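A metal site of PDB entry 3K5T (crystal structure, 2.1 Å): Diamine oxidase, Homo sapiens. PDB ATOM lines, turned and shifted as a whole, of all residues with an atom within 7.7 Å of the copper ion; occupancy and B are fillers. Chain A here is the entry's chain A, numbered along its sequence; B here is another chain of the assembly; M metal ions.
Of the 24 residues printed, 4 come within 4 Å of the copper ion.
The nearest printed residue that does not touch the copper ion is Phe 653 (4.8 Å).
The copper ion is bound by ND1 of His 655, NE2 of His 492, NE2 of His 490 and O4 of TPQ 441.
The copper ion has four donor atoms within binding distance.
A ring nitrogen (NE2) of His 655 is in hydrogen-bond range of the side-chain carboxylate of Asp 661 (3.3 Å).
The backbone carbonyl oxygen (O) of Phe 653 is in hydrogen-bond range of the backbone NH (N) of His 492 (2.6 Å).
ND1 of His 490 is in hydrogen-bond range of O of Asn 488 (2.8 Å).
O5 of TPQ 441 is in hydrogen-bond range of the side-chain hydroxyl (OG1) of Thr 665 (2.7 Å).
A ring nitrogen (ND1) of His 492 sits close to the side-chain hydroxyl (OH) of Tyr 443.
O2 of TPQ 441 lies close to the side-chain amide nitrogen of Asn 440 (3.4 Å).
O2 of TPQ 441 sits at hydrogen-bond distance from the side-chain hydroxyl (OH) of Tyr 443, 3.3 Å away.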
ATOM      1  N   ALA A 337       1.762   0.091 -23.449  1.00  0.00           N
ATOM      2  CA  ALA A 337       2.828  -0.519 -22.673  1.00  0.00           C
ATOM      3  C   ALA A 337       2.975  -1.958 -23.166  1.00  0.00           C
ATOM      4  O   ALA A 337       2.116  -2.784 -22.958  1.00  0.00           O
ATOM      5  CB  ALA A 337       2.507  -0.475 -21.170  1.00  0.00           C
ATOM      6  N   TYR A 339       5.099  -5.408 -23.266  1.00  0.00           N
ATOM      7  CA  TYR A 339       6.016  -6.144 -22.386  1.00  0.00           C
ATOM      8  C   TYR A 339       6.562  -7.440 -22.978  1.00  0.00           C
ATOM      9  O   TYR A 339       6.005  -8.000 -23.930  1.00  0.00           O
ATOM     10  CB  TYR A 339       5.288  -6.520 -21.098  1.00  0.00           C
ATOM     11  CG  TYR A 339       4.877  -5.364 -20.228  1.00  0.00           C
ATOM     12  CD1 TYR A 339       5.595  -5.037 -19.090  1.00  0.00           C
ATOM     13  CD2 TYR A 339       3.746  -4.613 -20.532  1.00  0.00           C
ATOM     14  CE1 TYR A 339       5.210  -3.971 -18.275  1.00  0.00           C
ATOM     15  CE2 TYR A 339       3.342  -3.543 -19.727  1.00  0.00           C
ATOM     16  CZ  TYR A 339       4.087  -3.238 -18.588  1.00  0.00           C
ATOM     17  OH  TYR A 339       3.695  -2.190 -17.763  1.00  0.00           O
ATOM     18  N   ASN A 440      -2.388   0.115 -12.232  1.00  0.00           N
ATOM     19  CA  ASN A 440      -1.111   0.266 -11.546  1.00  0.00           C
ATOM     20  C   ASN A 440      -0.396   1.584 -11.820  1.00  0.00           C
ATOM     21  O   ASN A 440       0.201   2.153 -10.910  1.00  0.00           O
ATOM     22  CB  ASN A 440      -0.144  -0.854 -11.964  1.00  0.00           C
ATOM     23  CG  ASN A 440       0.055  -0.922 -13.464  1.00  0.00           C
ATOM     24  OD1 ASN A 440      -0.915  -0.977 -14.215  1.00  0.00           O
ATOM     25  ND2 ASN A 440       1.308  -0.905 -13.923  1.00  0.00           N
ATOM     26  N   TPQ A 441      -0.466   2.044 -13.073  1.00  0.00           N
ATOM     27  CA  TPQ A 441       0.305   3.189 -13.563  1.00  0.00           C
ATOM     28  CB  TPQ A 441       0.666   3.082 -15.069  1.00  0.00           C
ATOM     29  C   TPQ A 441      -0.468   4.489 -13.413  1.00  0.00           C
ATOM     30  O   TPQ A 441      -1.682   4.513 -13.582  1.00  0.00           O
ATOM     31  C1  TPQ A 441       2.060   2.511 -15.290  1.00  0.00           C
ATOM     32  C2  TPQ A 441       2.290   1.381 -16.232  1.00  0.00           C
ATOM     33  O2  TPQ A 441       1.324   0.866 -16.858  1.00  0.00           O
ATOM     34  C3  TPQ A 441       3.670   0.852 -16.398  1.00  0.00           C
ATOM     35  C4  TPQ A 441       4.746   1.408 -15.702  1.00  0.00           C
ATOM     36  O4  TPQ A 441       5.917   0.968 -15.854  1.00  0.00           O
ATOM     37  C5  TPQ A 441       4.517   2.555 -14.785  1.00  0.00           C
ATOM     38  O5  TPQ A 441       5.458   3.068 -14.143  1.00  0.00           O
ATOM     39  C6  TPQ A 441       3.142   3.064 -14.615  1.00  0.00           C
ATOM     40  N   TYR A 443      -0.317   8.167 -15.166  1.00  0.00           N
ATOM     41  CA  TYR A 443       0.220   9.097 -16.167  1.00  0.00           C
ATOM     42  C   TYR A 443      -0.321  10.510 -15.919  1.00  0.00           C
ATOM     43  O   TYR A 443      -1.542  10.735 -15.842  1.00  0.00           O
ATOM     44  CB  TYR A 443      -0.081   8.628 -17.596  1.00  0.00           C
ATOM     45  CG  TYR A 443       0.474   7.238 -17.932  1.00  0.00           C
ATOM     46  CD1 TYR A 443       1.774   6.869 -17.582  1.00  0.00           C
ATOM     47  CD2 TYR A 443      -0.313   6.314 -18.603  1.00  0.00           C
ATOM     48  CE1 TYR A 443       2.266   5.605 -17.894  1.00  0.00           C
ATOM     49  CE2 TYR A 443       0.170   5.056 -18.923  1.00  0.00           C
ATOM     50  CZ  TYR A 443       1.443   4.700 -18.568  1.00  0.00           C
ATOM     51  OH  TYR A 443       1.888   3.432 -18.897  1.00  0.00           O
ATOM     52  N   ALA A 461       5.354   9.469 -16.351  1.00  0.00           N
ATOM     53  CA  ALA A 461       4.876   8.213 -15.797  1.00  0.00           C
ATOM     54  C   ALA A 461       5.294   8.081 -14.328  1.00  0.00           C
ATOM     55  O   ALA A 461       6.448   8.384 -13.938  1.00  0.00           O
ATOM     56  CB  ALA A 461       5.399   7.033 -16.614  1.00  0.00           C
ATOM     57  N   THR A 462       4.338   7.660 -13.513  1.00  0.00           N
ATOM     58  CA  THR A 462       4.639   7.265 -12.140  1.00  0.00           C
ATOM     59  C   THR A 462       3.653   6.163 -11.697  1.00  0.00           C
ATOM     60  O   THR A 462       2.952   5.597 -12.523  1.00  0.00           O
ATOM     61  CB  THR A 462       4.627   8.510 -11.173  1.00  0.00           C
ATOM     62  OG1 THR A 462       4.951   8.103  -9.835  1.00  0.00           O
ATOM     63  CG2 THR A 462       3.298   9.205 -11.196  1.00  0.00           C
ATOM     64  N   TYR A 464       2.606   2.410  -9.940  1.00  0.00           N
ATOM     65  CA  TYR A 464       3.171   1.058  -9.816  1.00  0.00           C
ATOM     66  C   TYR A 464       3.495   0.422 -11.165  1.00  0.00           C
ATOM     67  O   TYR A 464       2.695   0.477 -12.091  1.00  0.00           O
ATOM     68  CB  TYR A 464       2.198   0.131  -9.048  1.00  0.00           C
ATOM     69  CG  TYR A 464       2.134   0.414  -7.566  1.00  0.00           C
ATOM     70  CD1 TYR A 464       1.176   1.263  -7.040  1.00  0.00           C
ATOM     71  CD2 TYR A 464       3.037  -0.183  -6.701  1.00  0.00           C
ATOM     72  CE1 TYR A 464       1.107   1.514  -5.681  1.00  0.00           C
ATOM     73  CE2 TYR A 464       2.981   0.065  -5.347  1.00  0.00           C
ATOM     74  CZ  TYR A 464       2.016   0.914  -4.838  1.00  0.00           C
ATOM     75  OH  TYR A 464       1.983   1.154  -3.481  1.00  0.00           O
ATOM     76  N   VAL A 465       4.663  -0.211 -11.257  1.00  0.00           N
ATOM     77  CA  VAL A 465       5.040  -0.967 -12.457  1.00  0.00           C
ATOM     78  C   VAL A 465       4.224  -2.257 -12.563  1.00  0.00           C
ATOM     79  O   VAL A 465       3.618  -2.701 -11.577  1.00  0.00           O
ATOM     80  CB  VAL A 465       6.558  -1.298 -12.497  1.00  0.00           C
ATOM     81  CG1 VAL A 465       7.350  -0.023 -12.457  1.00  0.00           C
ATOM     82  CG2 VAL A 465       6.974  -2.249 -11.353  1.00  0.00           C
ATOM     83  N   HIS A 466       4.172  -2.809 -13.770  1.00  0.00           N
ATOM     84  CA  HIS A 466       3.468  -4.060 -14.038  1.00  0.00           C
ATOM     85  C   HIS A 466       4.481  -5.178 -13.834  1.00  0.00           C
ATOM     86  O   HIS A 466       5.495  -5.216 -14.529  1.00  0.00           O
ATOM     87  CB  HIS A 466       2.886  -4.037 -15.447  1.00  0.00           C
ATOM     88  CG  HIS A 466       2.324  -5.355 -15.919  1.00  0.00           C
ATOM     89  ND1 HIS A 466       1.210  -5.942 -15.366  1.00  0.00           N
ATOM     90  CD2 HIS A 466       2.693  -6.155 -16.946  1.00  0.00           C
ATOM     91  CE1 HIS A 466       0.941  -7.067 -16.006  1.00  0.00           C
ATOM     92  NE2 HIS A 466       1.828  -7.224 -16.971  1.00  0.00           N
ATOM     93  N   ASN A 488       8.920  -6.591 -15.180  1.00  0.00           N
ATOM     94  CA  ASN A 488       9.006  -6.908 -16.627  1.00  0.00           C
ATOM     95  C   ASN A 488       9.469  -5.759 -17.530  1.00  0.00           C
ATOM     96  O   ASN A 488       9.009  -4.610 -17.357  1.00  0.00           O
ATOM     97  CB  ASN A 488       7.652  -7.398 -17.167  1.00  0.00           C
ATOM     98  CG  ASN A 488       7.171  -8.648 -16.474  1.00  0.00           C
ATOM     99  OD1 ASN A 488       6.821  -8.611 -15.292  1.00  0.00           O
ATOM    100  ND2 ASN A 488       7.113  -9.755 -17.217  1.00  0.00           N
ATOM    101  N   ILE A 489      10.327  -6.081 -18.493  1.00  0.00           N
ATOM    102  CA  ILE A 489      10.776  -5.142 -19.538  1.00  0.00           C
ATOM    103  C   ILE A 489       9.607  -4.711 -20.386  1.00  0.00           C
ATOM    104  O   ILE A 489       8.701  -5.522 -20.680  1.00  0.00           O
ATOM    105  CB  ILE A 489      11.883  -5.762 -20.478  1.00  0.00           C
ATOM    106  CG1 ILE A 489      12.514  -4.688 -21.371  1.00  0.00           C
ATOM    107  CG2 ILE A 489      11.305  -6.855 -21.380  1.00  0.00           C
ATOM    108  CD1 ILE A 489      13.893  -5.084 -21.922  1.00  0.00           C
ATOM    109  N   HIS A 490       9.604  -3.430 -20.776  1.00  0.00           N
ATOM    110  CA  HIS A 490       8.539  -2.914 -21.627  1.00  0.00           C
ATOM    111  C   HIS A 490       8.875  -1.566 -22.271  1.00  0.00           C
ATOM    112  O   HIS A 490       9.778  -0.835 -21.868  1.00  0.00           O
ATOM    113  CB  HIS A 490       7.243  -2.790 -20.831  1.00  0.00           C
ATOM    114  CG  HIS A 490       7.350  -1.883 -19.646  1.00  0.00           C
ATOM    115  ND1 HIS A 490       8.160  -2.176 -18.570  1.00  0.00           N
ATOM    116  CD2 HIS A 490       6.790  -0.679 -19.386  1.00  0.00           C
ATOM    117  CE1 HIS A 490       8.071  -1.198 -17.679  1.00  0.00           C
ATOM    118  NE2 HIS A 490       7.264  -0.274 -18.163  1.00  0.00           N
ATOM    119  N   THR A 491       8.097  -1.219 -23.281  1.00  0.00           N
ATOM    120  CA  THR A 491       8.247   0.053 -23.951  1.00  0.00           C
ATOM    121  C   THR A 491       7.005   0.891 -23.699  1.00  0.00           C
ATOM    122  O   THR A 491       5.876   0.391 -23.870  1.00  0.00           O
ATOM    123  CB  THR A 491       8.481  -0.138 -25.451  1.00  0.00           C
ATOM    124  OG1 THR A 491       9.818  -0.612 -25.637  1.00  0.00           O
ATOM    125  CG2 THR A 491       8.335   1.193 -26.202  1.00  0.00           C
ATOM    126  N   HIS A 492       7.204   2.122 -23.257  1.00  0.00           N
ATOM    127  CA  HIS A 492       6.107   3.083 -23.227  1.00  0.00           C
ATOM    128  C   HIS A 492       6.101   3.862 -24.551  1.00  0.00           C
ATOM    129  O   HIS A 492       7.106   4.462 -24.925  1.00  0.00           O
ATOM    130  CB  HIS A 492       6.264   4.061 -22.072  1.00  0.00           C
ATOM    131  CG  HIS A 492       6.068   3.447 -20.719  1.00  0.00           C
ATOM    132  ND1 HIS A 492       4.818   3.178 -20.195  1.00  0.00           N
ATOM    133  CD2 HIS A 492       6.965   3.098 -19.761  1.00  0.00           C
ATOM    134  CE1 HIS A 492       4.964   2.671 -18.979  1.00  0.00           C
ATOM    135  NE2 HIS A 492       6.244   2.616 -18.694  1.00  0.00           N
ATOM    136  N   PHE A 653       9.514   5.515 -24.516  1.00  0.00           N
ATOM    137  CA  PHE A 653      10.780   5.108 -23.930  1.00  0.00           C
ATOM    138  C   PHE A 653      10.728   3.631 -23.475  1.00  0.00           C
ATOM    139  O   PHE A 653       9.653   3.094 -23.059  1.00  0.00           O
ATOM    140  CB  PHE A 653      11.205   6.067 -22.802  1.00  0.00           C
ATOM    141  CG  PHE A 653      10.299   6.047 -21.587  1.00  0.00           C
ATOM    142  CD1 PHE A 653      10.576   5.224 -20.504  1.00  0.00           C
ATOM    143  CD2 PHE A 653       9.157   6.851 -21.541  1.00  0.00           C
ATOM    144  CE1 PHE A 653       9.726   5.204 -19.395  1.00  0.00           C
ATOM    145  CE2 PHE A 653       8.319   6.835 -20.443  1.00  0.00           C
ATOM    146  CZ  PHE A 653       8.595   6.020 -19.367  1.00  0.00           C
ATOM    147  N   LEU A 654      11.885   2.999 -23.612  1.00  0.00           N
ATOM    148  CA  LEU A 654      12.133   1.640 -23.125  1.00  0.00           C
ATOM    149  C   LEU A 654      12.283   1.703 -21.612  1.00  0.00           C
ATOM    150  O   LEU A 654      13.173   2.378 -21.083  1.00  0.00           O
ATOM    151  CB  LEU A 654      13.414   1.081 -23.744  1.00  0.00           C
ATOM    152  CG  LEU A 654      13.911  -0.264 -23.158  1.00  0.00           C
ATOM    153  CD1 LEU A 654      12.900  -1.370 -23.376  1.00  0.00           C
ATOM    154  CD2 LEU A 654      15.285  -0.630 -23.719  1.00  0.00           C
ATOM    155  N   HIS A 655      11.412   1.002 -20.911  1.00  0.00           N
ATOM    156  CA  HIS A 655      11.485   0.973 -19.458  1.00  0.00           C
ATOM    157  C   HIS A 655      11.971  -0.389 -18.941  1.00  0.00           C
ATOM    158  O   HIS A 655      11.217  -1.354 -18.928  1.00  0.00           O
ATOM    159  CB  HIS A 655      10.128   1.334 -18.872  1.00  0.00           C
ATOM    160  CG  HIS A 655      10.137   1.542 -17.382  1.00  0.00           C
ATOM    161  ND1 HIS A 655       8.982   1.728 -16.673  1.00  0.00           N
ATOM    162  CD2 HIS A 655      11.151   1.587 -16.487  1.00  0.00           C
ATOM    163  CE1 HIS A 655       9.266   1.852 -15.395  1.00  0.00           C
ATOM    164  NE2 HIS A 655      10.584   1.780 -15.252  1.00  0.00           N
ATOM    165  N   ILE A 656      13.234  -0.461 -18.560  1.00  0.00           N
ATOM    166  CA  ILE A 656      13.731  -1.633 -17.863  1.00  0.00           C
ATOM    167  C   ILE A 656      13.598  -1.389 -16.357  1.00  0.00           C
ATOM    168  O   ILE A 656      14.404  -0.641 -15.786  1.00  0.00           O
ATOM    169  CB  ILE A 656      15.186  -1.951 -18.241  1.00  0.00           C
ATOM    170  CG1 ILE A 656      15.319  -2.232 -19.746  1.00  0.00           C
ATOM    171  CG2 ILE A 656      15.684  -3.183 -17.474  1.00  0.00           C
ATOM    172  CD1 ILE A 656      16.748  -2.173 -20.238  1.00  0.00           C
ATOM    173  N   PRO A 657      12.611  -2.024 -15.701  1.00  0.00           N
ATOM    174  CA  PRO A 657      12.481  -1.808 -14.265  1.00  0.00           C
ATOM    175  C   PRO A 657      13.774  -1.965 -13.456  1.00  0.00           C
ATOM    176  O   PRO A 657      14.604  -2.796 -13.775  1.00  0.00           O
ATOM    177  CB  PRO A 657      11.455  -2.851 -13.856  1.00  0.00           C
ATOM    178  CG  PRO A 657      10.487  -2.826 -15.029  1.00  0.00           C
ATOM    179  CD  PRO A 657      11.446  -2.784 -16.224  1.00  0.00           C
ATOM    180  N   ASP A 661      12.349   1.644  -8.742  1.00  0.00           N
ATOM    181  CA  ASP A 661      10.923   1.670  -9.095  1.00  0.00           C
ATOM    182  C   ASP A 661      10.008   1.112  -8.019  1.00  0.00           C
ATOM    183  O   ASP A 661       8.822   0.953  -8.265  1.00  0.00           O
ATOM    184  CB  ASP A 661      10.671   0.845 -10.350  1.00  0.00           C
ATOM    185  CG  ASP A 661      11.252   1.467 -11.579  1.00  0.00           C
ATOM    186  OD1 ASP A 661      11.149   2.703 -11.719  1.00  0.00           O
ATOM    187  OD2 ASP A 661      11.797   0.722 -12.426  1.00  0.00           O
ATOM    188  N   THR A 665       7.432   3.882  -9.719  1.00  0.00           N
ATOM    189  CA  THR A 665       8.229   4.602 -10.716  1.00  0.00           C
ATOM    190  C   THR A 665       8.165   6.079 -10.397  1.00  0.00           C
ATOM    191  O   THR A 665       7.089   6.605 -10.161  1.00  0.00           O
ATOM    192  CB  THR A 665       7.668   4.418 -12.150  1.00  0.00           C
ATOM    193  OG1 THR A 665       7.555   3.026 -12.450  1.00  0.00           O
ATOM    194  CG2 THR A 665       8.602   5.079 -13.161  1.00  0.00           C
ATOM    195  N   ASN A 670      11.341  10.593 -16.393  1.00  0.00           N
ATOM    196  CA  ASN A 670      10.419   9.564 -16.903  1.00  0.00           C
ATOM    197  C   ASN A 670       9.300  10.307 -17.614  1.00  0.00           C
ATOM    198  O   ASN A 670       8.128  10.075 -17.331  1.00  0.00           O
ATOM    199  CB  ASN A 670       9.855   8.681 -15.752  1.00  0.00           C
ATOM    200  CG  ASN A 670      10.732   7.435 -15.450  1.00  0.00           C
ATOM    201  OD1 ASN A 670      11.189   6.743 -16.347  1.00  0.00           O
ATOM    202  ND2 ASN A 670      10.943   7.153 -14.147  1.00  0.00           N
ATOM    203  N   TYR B 556      20.097   2.298 -22.868  1.00  0.00           N
ATOM    204  CA  TYR B 556      20.531   2.255 -21.482  1.00  0.00           C
ATOM    205  C   TYR B 556      22.038   2.276 -21.441  1.00  0.00           C
ATOM    206  O   TYR B 556      22.668   1.368 -21.950  1.00  0.00           O
ATOM    207  CB  TYR B 556      19.999   1.005 -20.799  1.00  0.00           C
ATOM    208  CG  TYR B 556      18.608   1.181 -20.251  1.00  0.00           C
ATOM    209  CD1 TYR B 556      17.497   1.075 -21.066  1.00  0.00           C
ATOM    210  CD2 TYR B 556      18.406   1.497 -18.906  1.00  0.00           C
ATOM    211  CE1 TYR B 556      16.211   1.260 -20.571  1.00  0.00           C
ATOM    212  CE2 TYR B 556      17.140   1.680 -18.400  1.00  0.00           C
ATOM    213  CZ  TYR B 556      16.045   1.573 -19.234  1.00  0.00           C
ATOM    214  OH  TYR B 556      14.789   1.751 -18.720  1.00  0.00           O
HETATM  215 CU    CU M   1       7.306   1.608 -17.332  1.00  0.00          CU
